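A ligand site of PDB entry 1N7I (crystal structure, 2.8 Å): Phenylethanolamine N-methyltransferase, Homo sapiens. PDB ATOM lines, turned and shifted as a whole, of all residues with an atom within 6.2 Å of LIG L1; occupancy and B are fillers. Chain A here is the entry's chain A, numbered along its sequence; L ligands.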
ATOM      1  N   TYR A  35       8.522  10.361 -19.820  1.00  0.00           N
ATOM      2  CA  TYR A  35       9.294  11.137 -18.879  1.00  0.00           C
ATOM      3  C   TYR A  35       9.209  12.600 -19.310  1.00  0.00           C
ATOM      4  O   TYR A  35       8.705  13.448 -18.562  1.00  0.00           O
ATOM      5  CB  TYR A  35      10.754  10.714 -18.898  1.00  0.00           C
ATOM      6  CG  TYR A  35      11.621  11.585 -18.014  1.00  0.00           C
ATOM      7  CD1 TYR A  35      11.654  11.381 -16.631  1.00  0.00           C
ATOM      8  CD2 TYR A  35      12.394  12.608 -18.554  1.00  0.00           C
ATOM      9  CE1 TYR A  35      12.450  12.191 -15.811  1.00  0.00           C
ATOM     10  CE2 TYR A  35      13.181  13.418 -17.744  1.00  0.00           C
ATOM     11  CZ  TYR A  35      13.208  13.199 -16.376  1.00  0.00           C
ATOM     12  OH  TYR A  35      14.017  13.972 -15.588  1.00  0.00           O
ATOM     13  N   ASN A  39       7.536  16.158 -17.258  1.00  0.00           N
ATOM     14  CA  ASN A  39       8.373  17.216 -16.710  1.00  0.00           C
ATOM     15  C   ASN A  39       8.734  18.368 -17.633  1.00  0.00           C
ATOM     16  O   ASN A  39       9.193  19.407 -17.155  1.00  0.00           O
ATOM     17  CB  ASN A  39       9.654  16.598 -16.173  1.00  0.00           C
ATOM     18  CG  ASN A  39       9.379  15.465 -15.244  1.00  0.00           C
ATOM     19  OD1 ASN A  39       8.937  15.670 -14.132  1.00  0.00           O
ATOM     20  ND2 ASN A  39       9.623  14.257 -15.709  1.00  0.00           N
ATOM     21  N   TYR A  40       8.545  18.201 -18.932  1.00  0.00           N
ATOM     22  CA  TYR A  40       8.909  19.263 -19.862  1.00  0.00           C
ATOM     23  C   TYR A  40       7.819  19.664 -20.817  1.00  0.00           C
ATOM     24  O   TYR A  40       8.106  20.184 -21.903  1.00  0.00           O
ATOM     25  CB  TYR A  40      10.168  18.866 -20.628  1.00  0.00           C
ATOM     26  CG  TYR A  40      11.292  18.565 -19.691  1.00  0.00           C
ATOM     27  CD1 TYR A  40      11.423  17.307 -19.098  1.00  0.00           C
ATOM     28  CD2 TYR A  40      12.193  19.557 -19.335  1.00  0.00           C
ATOM     29  CE1 TYR A  40      12.432  17.049 -18.176  1.00  0.00           C
ATOM     30  CE2 TYR A  40      13.198  19.315 -18.408  1.00  0.00           C
ATOM     31  CZ  TYR A  40      13.316  18.065 -17.832  1.00  0.00           C
ATOM     32  OH  TYR A  40      14.335  17.830 -16.937  1.00  0.00           O
ATOM     33  N   ARG A  44       4.757  22.323 -16.430  1.00  0.00           N
ATOM     34  CA  ARG A  44       6.168  22.536 -16.147  1.00  0.00           C
ATOM     35  C   ARG A  44       6.948  23.013 -17.348  1.00  0.00           C
ATOM     36  O   ARG A  44       7.958  23.708 -17.198  1.00  0.00           O
ATOM     37  CB  ARG A  44       6.805  21.256 -15.620  1.00  0.00           C
ATOM     38  CG  ARG A  44       6.180  20.756 -14.355  1.00  0.00           C
ATOM     39  CD  ARG A  44       6.936  19.581 -13.790  1.00  0.00           C
ATOM     40  NE  ARG A  44       6.337  19.201 -12.515  1.00  0.00           N
ATOM     41  CZ  ARG A  44       6.724  18.160 -11.786  1.00  0.00           C
ATOM     42  NH1 ARG A  44       7.709  17.373 -12.198  1.00  0.00           N
ATOM     43  NH2 ARG A  44       6.109  17.917 -10.637  1.00  0.00           N
ATOM     44  N   VAL A  53       9.317  26.331 -13.067  1.00  0.00           N
ATOM     45  CA  VAL A  53      10.554  25.574 -12.907  1.00  0.00           C
ATOM     46  C   VAL A  53      11.447  25.817 -14.097  1.00  0.00           C
ATOM     47  O   VAL A  53      12.659  25.970 -13.951  1.00  0.00           O
ATOM     48  CB  VAL A  53      10.320  24.038 -12.849  1.00  0.00           C
ATOM     49  CG1 VAL A  53      11.384  23.392 -11.948  1.00  0.00           C
ATOM     50  CG2 VAL A  53       8.923  23.721 -12.384  1.00  0.00           C
ATOM     51  N   GLY A  54      10.843  25.829 -15.282  1.00  0.00           N
ATOM     52  CA  GLY A  54      11.590  26.032 -16.502  1.00  0.00           C
ATOM     53  C   GLY A  54      12.422  27.302 -16.470  1.00  0.00           C
ATOM     54  O   GLY A  54      13.660  27.245 -16.513  1.00  0.00           O
ATOM     55  N   LYS A  57      15.273  27.170 -13.681  1.00  0.00           N
ATOM     56  CA  LYS A  57      16.452  26.400 -14.005  1.00  0.00           C
ATOM     57  C   LYS A  57      17.237  27.074 -15.112  1.00  0.00           C
ATOM     58  O   LYS A  57      18.464  27.225 -15.009  1.00  0.00           O
ATOM     59  CB  LYS A  57      16.088  24.982 -14.435  1.00  0.00           C
ATOM     60  CG  LYS A  57      15.480  24.115 -13.340  1.00  0.00           C
ATOM     61  CD  LYS A  57      15.103  22.742 -13.874  1.00  0.00           C
ATOM     62  CE  LYS A  57      13.940  22.857 -14.841  1.00  0.00           C
ATOM     63  NZ  LYS A  57      13.741  21.616 -15.598  1.00  0.00           N
ATOM     64  N   TYR A  85      18.032  20.981 -22.449  1.00  0.00           N
ATOM     65  CA  TYR A  85      17.937  22.263 -21.741  1.00  0.00           C
ATOM     66  C   TYR A  85      19.102  22.589 -20.805  1.00  0.00           C
ATOM     67  O   TYR A  85      19.392  23.760 -20.550  1.00  0.00           O
ATOM     68  CB  TYR A  85      16.626  22.310 -20.940  1.00  0.00           C
ATOM     69  CG  TYR A  85      16.697  21.559 -19.638  1.00  0.00           C
ATOM     70  CD1 TYR A  85      17.193  22.171 -18.488  1.00  0.00           C
ATOM     71  CD2 TYR A  85      16.277  20.237 -19.540  1.00  0.00           C
ATOM     72  CE1 TYR A  85      17.290  21.485 -17.288  1.00  0.00           C
ATOM     73  CE2 TYR A  85      16.379  19.535 -18.344  1.00  0.00           C
ATOM     74  CZ  TYR A  85      16.875  20.170 -17.232  1.00  0.00           C
ATOM     75  OH  TYR A  85      16.982  19.487 -16.051  1.00  0.00           O
ATOM     76  N   PHE A 182      18.951  16.317 -12.149  1.00  0.00           N
ATOM     77  CA  PHE A 182      18.054  15.271 -11.697  1.00  0.00           C
ATOM     78  C   PHE A 182      18.599  13.851 -11.892  1.00  0.00           C
ATOM     79  O   PHE A 182      17.844  12.931 -12.199  1.00  0.00           O
ATOM     80  CB  PHE A 182      16.700  15.415 -12.411  1.00  0.00           C
ATOM     81  CG  PHE A 182      16.122  16.795 -12.323  1.00  0.00           C
ATOM     82  CD1 PHE A 182      16.262  17.686 -13.389  1.00  0.00           C
ATOM     83  CD2 PHE A 182      15.448  17.207 -11.186  1.00  0.00           C
ATOM     84  CE1 PHE A 182      15.724  18.975 -13.315  1.00  0.00           C
ATOM     85  CE2 PHE A 182      14.907  18.492 -11.099  1.00  0.00           C
ATOM     86  CZ  PHE A 182      15.047  19.383 -12.164  1.00  0.00           C
ATOM     87  N   ALA A 216      16.260  17.090  -7.487  1.00  0.00           N
ATOM     88  CA  ALA A 216      14.974  17.174  -6.836  1.00  0.00           C
ATOM     89  C   ALA A 216      15.214  17.280  -5.344  1.00  0.00           C
ATOM     90  O   ALA A 216      16.089  16.619  -4.792  1.00  0.00           O
ATOM     91  CB  ALA A 216      14.147  15.956  -7.136  1.00  0.00           C
ATOM     92  N   GLU A 219      12.271  14.634  -2.684  1.00  0.00           N
ATOM     93  CA  GLU A 219      11.343  13.850  -3.515  1.00  0.00           C
ATOM     94  C   GLU A 219      11.687  12.375  -3.274  1.00  0.00           C
ATOM     95  O   GLU A 219      12.834  12.061  -2.929  1.00  0.00           O
ATOM     96  CB  GLU A 219      11.471  14.214  -5.015  1.00  0.00           C
ATOM     97  CG  GLU A 219      12.444  13.353  -5.812  1.00  0.00           C
ATOM     98  CD  GLU A 219      12.202  13.413  -7.324  1.00  0.00           C
ATOM     99  OE1 GLU A 219      11.028  13.493  -7.742  1.00  0.00           O
ATOM    100  OE2 GLU A 219      13.196  13.355  -8.105  1.00  0.00           O
ATOM    101  N   TRP A 221       9.972   9.630  -5.340  1.00  0.00           N
ATOM    102  CA  TRP A 221       9.553   8.787  -6.457  1.00  0.00           C
ATOM    103  C   TRP A 221       9.057   9.672  -7.579  1.00  0.00           C
ATOM    104  O   TRP A 221       8.704  10.829  -7.355  1.00  0.00           O
ATOM    105  CB  TRP A 221       8.419   7.851  -6.037  1.00  0.00           C
ATOM    106  CG  TRP A 221       7.147   8.567  -5.626  1.00  0.00           C
ATOM    107  CD1 TRP A 221       6.769   8.927  -4.374  1.00  0.00           C
ATOM    108  CD2 TRP A 221       6.105   9.058  -6.507  1.00  0.00           C
ATOM    109  NE1 TRP A 221       5.575   9.608  -4.402  1.00  0.00           N
ATOM    110  CE2 TRP A 221       5.147   9.704  -5.704  1.00  0.00           C
ATOM    111  CE3 TRP A 221       5.908   9.011  -7.889  1.00  0.00           C
ATOM    112  CZ2 TRP A 221       3.993  10.303  -6.237  1.00  0.00           C
ATOM    113  CZ3 TRP A 221       4.761   9.608  -8.429  1.00  0.00           C
ATOM    114  CH2 TRP A 221       3.819  10.248  -7.592  1.00  0.00           C
ATOM    115  N   TYR A 222       9.054   9.128  -8.798  1.00  0.00           N
ATOM    116  CA  TYR A 222       8.540   9.871  -9.958  1.00  0.00           C
ATOM    117  C   TYR A 222       8.270   8.887 -11.077  1.00  0.00           C
ATOM    118  O   TYR A 222       9.071   7.988 -11.339  1.00  0.00           O
ATOM    119  CB  TYR A 222       9.523  10.958 -10.413  1.00  0.00           C
ATOM    120  CG  TYR A 222      10.744  10.443 -11.099  1.00  0.00           C
ATOM    121  CD1 TYR A 222      10.707  10.110 -12.462  1.00  0.00           C
ATOM    122  CD2 TYR A 222      11.943  10.269 -10.414  1.00  0.00           C
ATOM    123  CE1 TYR A 222      11.836   9.628 -13.108  1.00  0.00           C
ATOM    124  CE2 TYR A 222      13.075   9.780 -11.054  1.00  0.00           C
ATOM    125  CZ  TYR A 222      13.014   9.461 -12.402  1.00  0.00           C
ATOM    126  OH  TYR A 222      14.111   8.944 -13.038  1.00  0.00           O
ATOM    127  N   MET A 258       8.547  24.099  -5.323  1.00  0.00           N
ATOM    128  CA  MET A 258       7.504  23.696  -6.253  1.00  0.00           C
ATOM    129  C   MET A 258       6.163  24.345  -5.946  1.00  0.00           C
ATOM    130  O   MET A 258       5.637  24.191  -4.858  1.00  0.00           O
ATOM    131  CB  MET A 258       7.375  22.173  -6.255  1.00  0.00           C
ATOM    132  CG  MET A 258       8.331  21.493  -7.225  1.00  0.00           C
ATOM    133  SD  MET A 258       8.055  21.996  -8.939  1.00  0.00           S
ATOM    134  CE  MET A 258       9.736  21.669  -9.715  1.00  0.00           C
ATOM    135  N   LEU A 262       2.312  23.309 -10.190  1.00  0.00           N
ATOM    136  CA  LEU A 262       3.323  22.481 -10.826  1.00  0.00           C
ATOM    137  C   LEU A 262       3.478  21.148 -10.122  1.00  0.00           C
ATOM    138  O   LEU A 262       4.377  20.357 -10.443  1.00  0.00           O
ATOM    139  CB  LEU A 262       4.674  23.213 -10.904  1.00  0.00           C
ATOM    140  CG  LEU A 262       4.692  24.384 -11.889  1.00  0.00           C
ATOM    141  CD1 LEU A 262       6.094  24.915 -12.015  1.00  0.00           C
ATOM    142  CD2 LEU A 262       4.177  23.942 -13.239  1.00  0.00           C
ATOM    143  N   VAL A 266       2.988  13.224 -11.057  1.00  0.00           N
ATOM    144  CA  VAL A 266       4.045  12.456 -11.714  1.00  0.00           C
ATOM    145  C   VAL A 266       5.213  12.215 -10.797  1.00  0.00           C
ATOM    146  O   VAL A 266       6.131  11.476 -11.133  1.00  0.00           O
ATOM    147  CB  VAL A 266       4.559  13.160 -12.991  1.00  0.00           C
ATOM    148  CG1 VAL A 266       3.391  13.546 -13.872  1.00  0.00           C
ATOM    149  CG2 VAL A 266       5.426  14.365 -12.632  1.00  0.00           C
ATOM    150  N   ASP A 267       5.185  12.864  -9.651  1.00  0.00           N
ATOM    151  CA  ASP A 267       6.245  12.721  -8.675  1.00  0.00           C
ATOM    152  C   ASP A 267       5.772  13.416  -7.424  1.00  0.00           C
ATOM    153  O   ASP A 267       4.637  13.885  -7.371  1.00  0.00           O
ATOM    154  CB  ASP A 267       7.539  13.355  -9.173  1.00  0.00           C
ATOM    155  CG  ASP A 267       7.363  14.792  -9.568  1.00  0.00           C
ATOM    156  OD1 ASP A 267       6.919  15.605  -8.732  1.00  0.00           O
ATOM    157  OD2 ASP A 267       7.668  15.128 -10.729  1.00  0.00           O
ATOM    158  N   VAL A 269       7.989  15.780  -5.749  1.00  0.00           N
ATOM    159  CA  VAL A 269       9.005  16.797  -5.493  1.00  0.00           C
ATOM    160  C   VAL A 269       8.412  17.929  -4.647  1.00  0.00           C
ATOM    161  O   VAL A 269       7.239  18.276  -4.809  1.00  0.00           O
ATOM    162  CB  VAL A 269       9.531  17.403  -6.825  1.00  0.00           C
ATOM    163  CG1 VAL A 269      10.746  18.261  -6.570  1.00  0.00           C
ATOM    164  CG2 VAL A 269       9.876  16.291  -7.785  1.00  0.00           C
ATOM    165  N   VAL A 272      13.289  22.395  -5.836  1.00  0.00           N
ATOM    166  CA  VAL A 272      14.430  21.999  -6.666  1.00  0.00           C
ATOM    167  C   VAL A 272      15.682  22.812  -6.371  1.00  0.00           C
ATOM    168  O   VAL A 272      15.631  24.025  -6.169  1.00  0.00           O
ATOM    169  CB  VAL A 272      14.092  22.131  -8.170  1.00  0.00           C
ATOM    170  CG1 VAL A 272      15.278  21.660  -8.998  1.00  0.00           C
ATOM    171  CG2 VAL A 272      12.860  21.323  -8.504  1.00  0.00           C
HETATM  172  C1  LIG L   1      11.287  16.481 -10.732  1.00  0.00           C
HETATM  173  N1  LIG L   1      10.463  15.270 -11.074  1.00  0.00           N
HETATM  174  C2  LIG L   1      11.301  14.094 -11.461  1.00  0.00           C
HETATM  175  C3  LIG L   1      11.982  14.284 -12.803  1.00  0.00           C
HETATM  176  C4  LIG L   1      12.992  15.425 -12.791  1.00  0.00           C
HETATM  177  C5  LIG L   1      12.384  16.787 -12.950  1.00  0.00           C
HETATM  178  C6  LIG L   1      12.671  17.509 -14.096  1.00  0.00           C
HETATM  179  C7  LIG L   1      12.113  18.771 -14.269  1.00  0.00           C
HETATM  180  C8  LIG L   1      11.284  19.337 -13.289  1.00  0.00           C
HETATM  181  C9  LIG L   1      10.985  18.611 -12.093  1.00  0.00           C
HETATM  182  C10 LIG L   1      11.562  17.319 -11.949  1.00  0.00           C
HETATM  183 CL1  LIG L   1      10.753  20.667 -13.593  1.00  0.00          CL
HETATM  184 CL2  LIG L   1      10.126  19.168 -10.978  1.00  0.00          CL
HETATM  185  N1  LG2 L   2      19.014  15.274 -16.692  1.00  0.00           N
HETATM  186  C1  LG2 L   2      17.795  14.802 -17.376  1.00  0.00           C
HETATM  187  C2  LG2 L   2      17.227  13.472 -16.880  1.00  0.00           C
HETATM  188  C3  LG2 L   2      17.149  13.309 -15.390  1.00  0.00           C
HETATM  189  S1  LG2 L   2      16.365  11.719 -15.120  1.00  0.00           S
HETATM  190  C4  LG2 L   2      16.794  15.951 -17.236  1.00  0.00           C
HETATM  191  O1  LG2 L   2      17.224  16.982 -16.622  1.00  0.00           O
HETATM  192  O2  LG2 L   2      15.643  15.617 -16.734  1.00  0.00           O
HETATM  193  C5  LG2 L   2      17.585  10.606 -14.370  1.00  0.00           C
HETATM  194  C6  LG2 L   2      18.486   9.945 -15.433  1.00  0.00           C
HETATM  195  O3  LG2 L   2      19.420   9.084 -14.819  1.00  0.00           O
HETATM  196  C7  LG2 L   2      17.732   9.075 -16.395  1.00  0.00           C
HETATM  197  O4  LG2 L   2      17.852   9.545 -17.735  1.00  0.00           O
HETATM  198  C8  LG2 L   2      18.360   7.712 -16.215  1.00  0.00           C
HETATM  199  O5  LG2 L   2      18.390   6.952 -17.407  1.00  0.00           O
HETATM  200  C9  LG2 L   2      19.732   8.050 -15.753  1.00  0.00           C
HETATM  201  N2  LG2 L   2      20.360   6.987 -15.021  1.00  0.00           N
HETATM  202  C10 LG2 L   2      19.767   5.835 -14.454  1.00  0.00           C
HETATM  203  N3  LG2 L   2      20.615   5.069 -13.860  1.00  0.00           N
HETATM  204  C11 LG2 L   2      21.833   5.736 -14.019  1.00  0.00           C
HETATM  205  C12 LG2 L   2      23.142   5.427 -13.614  1.00  0.00           C
HETATM  206  N4  LG2 L   2      23.435   4.328 -12.915  1.00  0.00           N
HETATM  207  N5  LG2 L   2      24.136   6.332 -13.959  1.00  0.00           N
HETATM  208  C13 LG2 L   2      23.868   7.460 -14.672  1.00  0.00           C
HETATM  209  N6  LG2 L   2      22.690   7.860 -15.111  1.00  0.00           N
HETATM  210  C14 LG2 L   2      21.704   6.921 -14.745  1.00  0.00           C
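OE1 of Glu 219 is in salt-bridge range of N1 of LIG L1, at 3.8 Å.
An oxygen (O2) of LG2 L2 sits at hydrogen-bond distance from the side-chain hydroxyl (OH) of Tyr 35, 2.6 Å away.
The side-chain hydroxyl of Tyr 40 sits at hydrogen-bond distance from an oxygen (O2) of LG2 L2, 2.6 Å away.
The side-chain carboxylate of Asp 267 lies within salt-bridge range of a nitrogen (N1) of LIG L1, at 2.8 Å.
OH of Tyr 85 sits at hydrogen-bond distance from O1 of LG2 L2 (2.6 Å).
The side-chain amide oxygen (OD1) of Asn 39 lies within hydrogen-bond range of a nitrogen (N1) of LIG L1.
The guanidinium group (NH1) of Arg 44 is in hydrogen-bond range of the side-chain amide oxygen (OD1) of Asn 39 (2.9 Å).
ND2 of Asn 39 is in hydrogen-bond range of O of Tyr 35.
The side-chain hydroxyl (OH) of Tyr 85 sits close to the side-chain hydroxyl (OH) of Tyr 40 (3.2 Å).
OD2 of Asp 267 lies within salt-bridge range of NH1 of Arg 44, 2.7 Å away.
NH2 of Arg 44 sits at hydrogen-bond distance from O of Leu 262 (3.0 Å).
The side-chain carboxylate (OD1) of Asp 267 is in hydrogen-bond range of the backbone NH (N) of Val 269 (3.2 Å).
Residues that only touch LIG L1: Tyr 35 (3.3 Å), Tyr 40 (3.3 Å), Arg 44 (3.2 Å), Val 53 (3.2 Å), Lys 57 (3.5 Å), Phe 182 (3.4 Å), Tyr 222 (3.7 Å), Met 258 (2.8 Å) and Val 269 (3.3 Å).
Hydrophobic or aromatic side chains within 4 Å of LIG L1: Tyr 35, Tyr 40, Val 53, Phe 182, Tyr 222, Met 258 and Val 269.
Of the 19 residues printed, 12 come within 4 Å of LIG L1.
The nearest printed residue that does not touch LIG L1 is Val 272 (4.3 Å).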
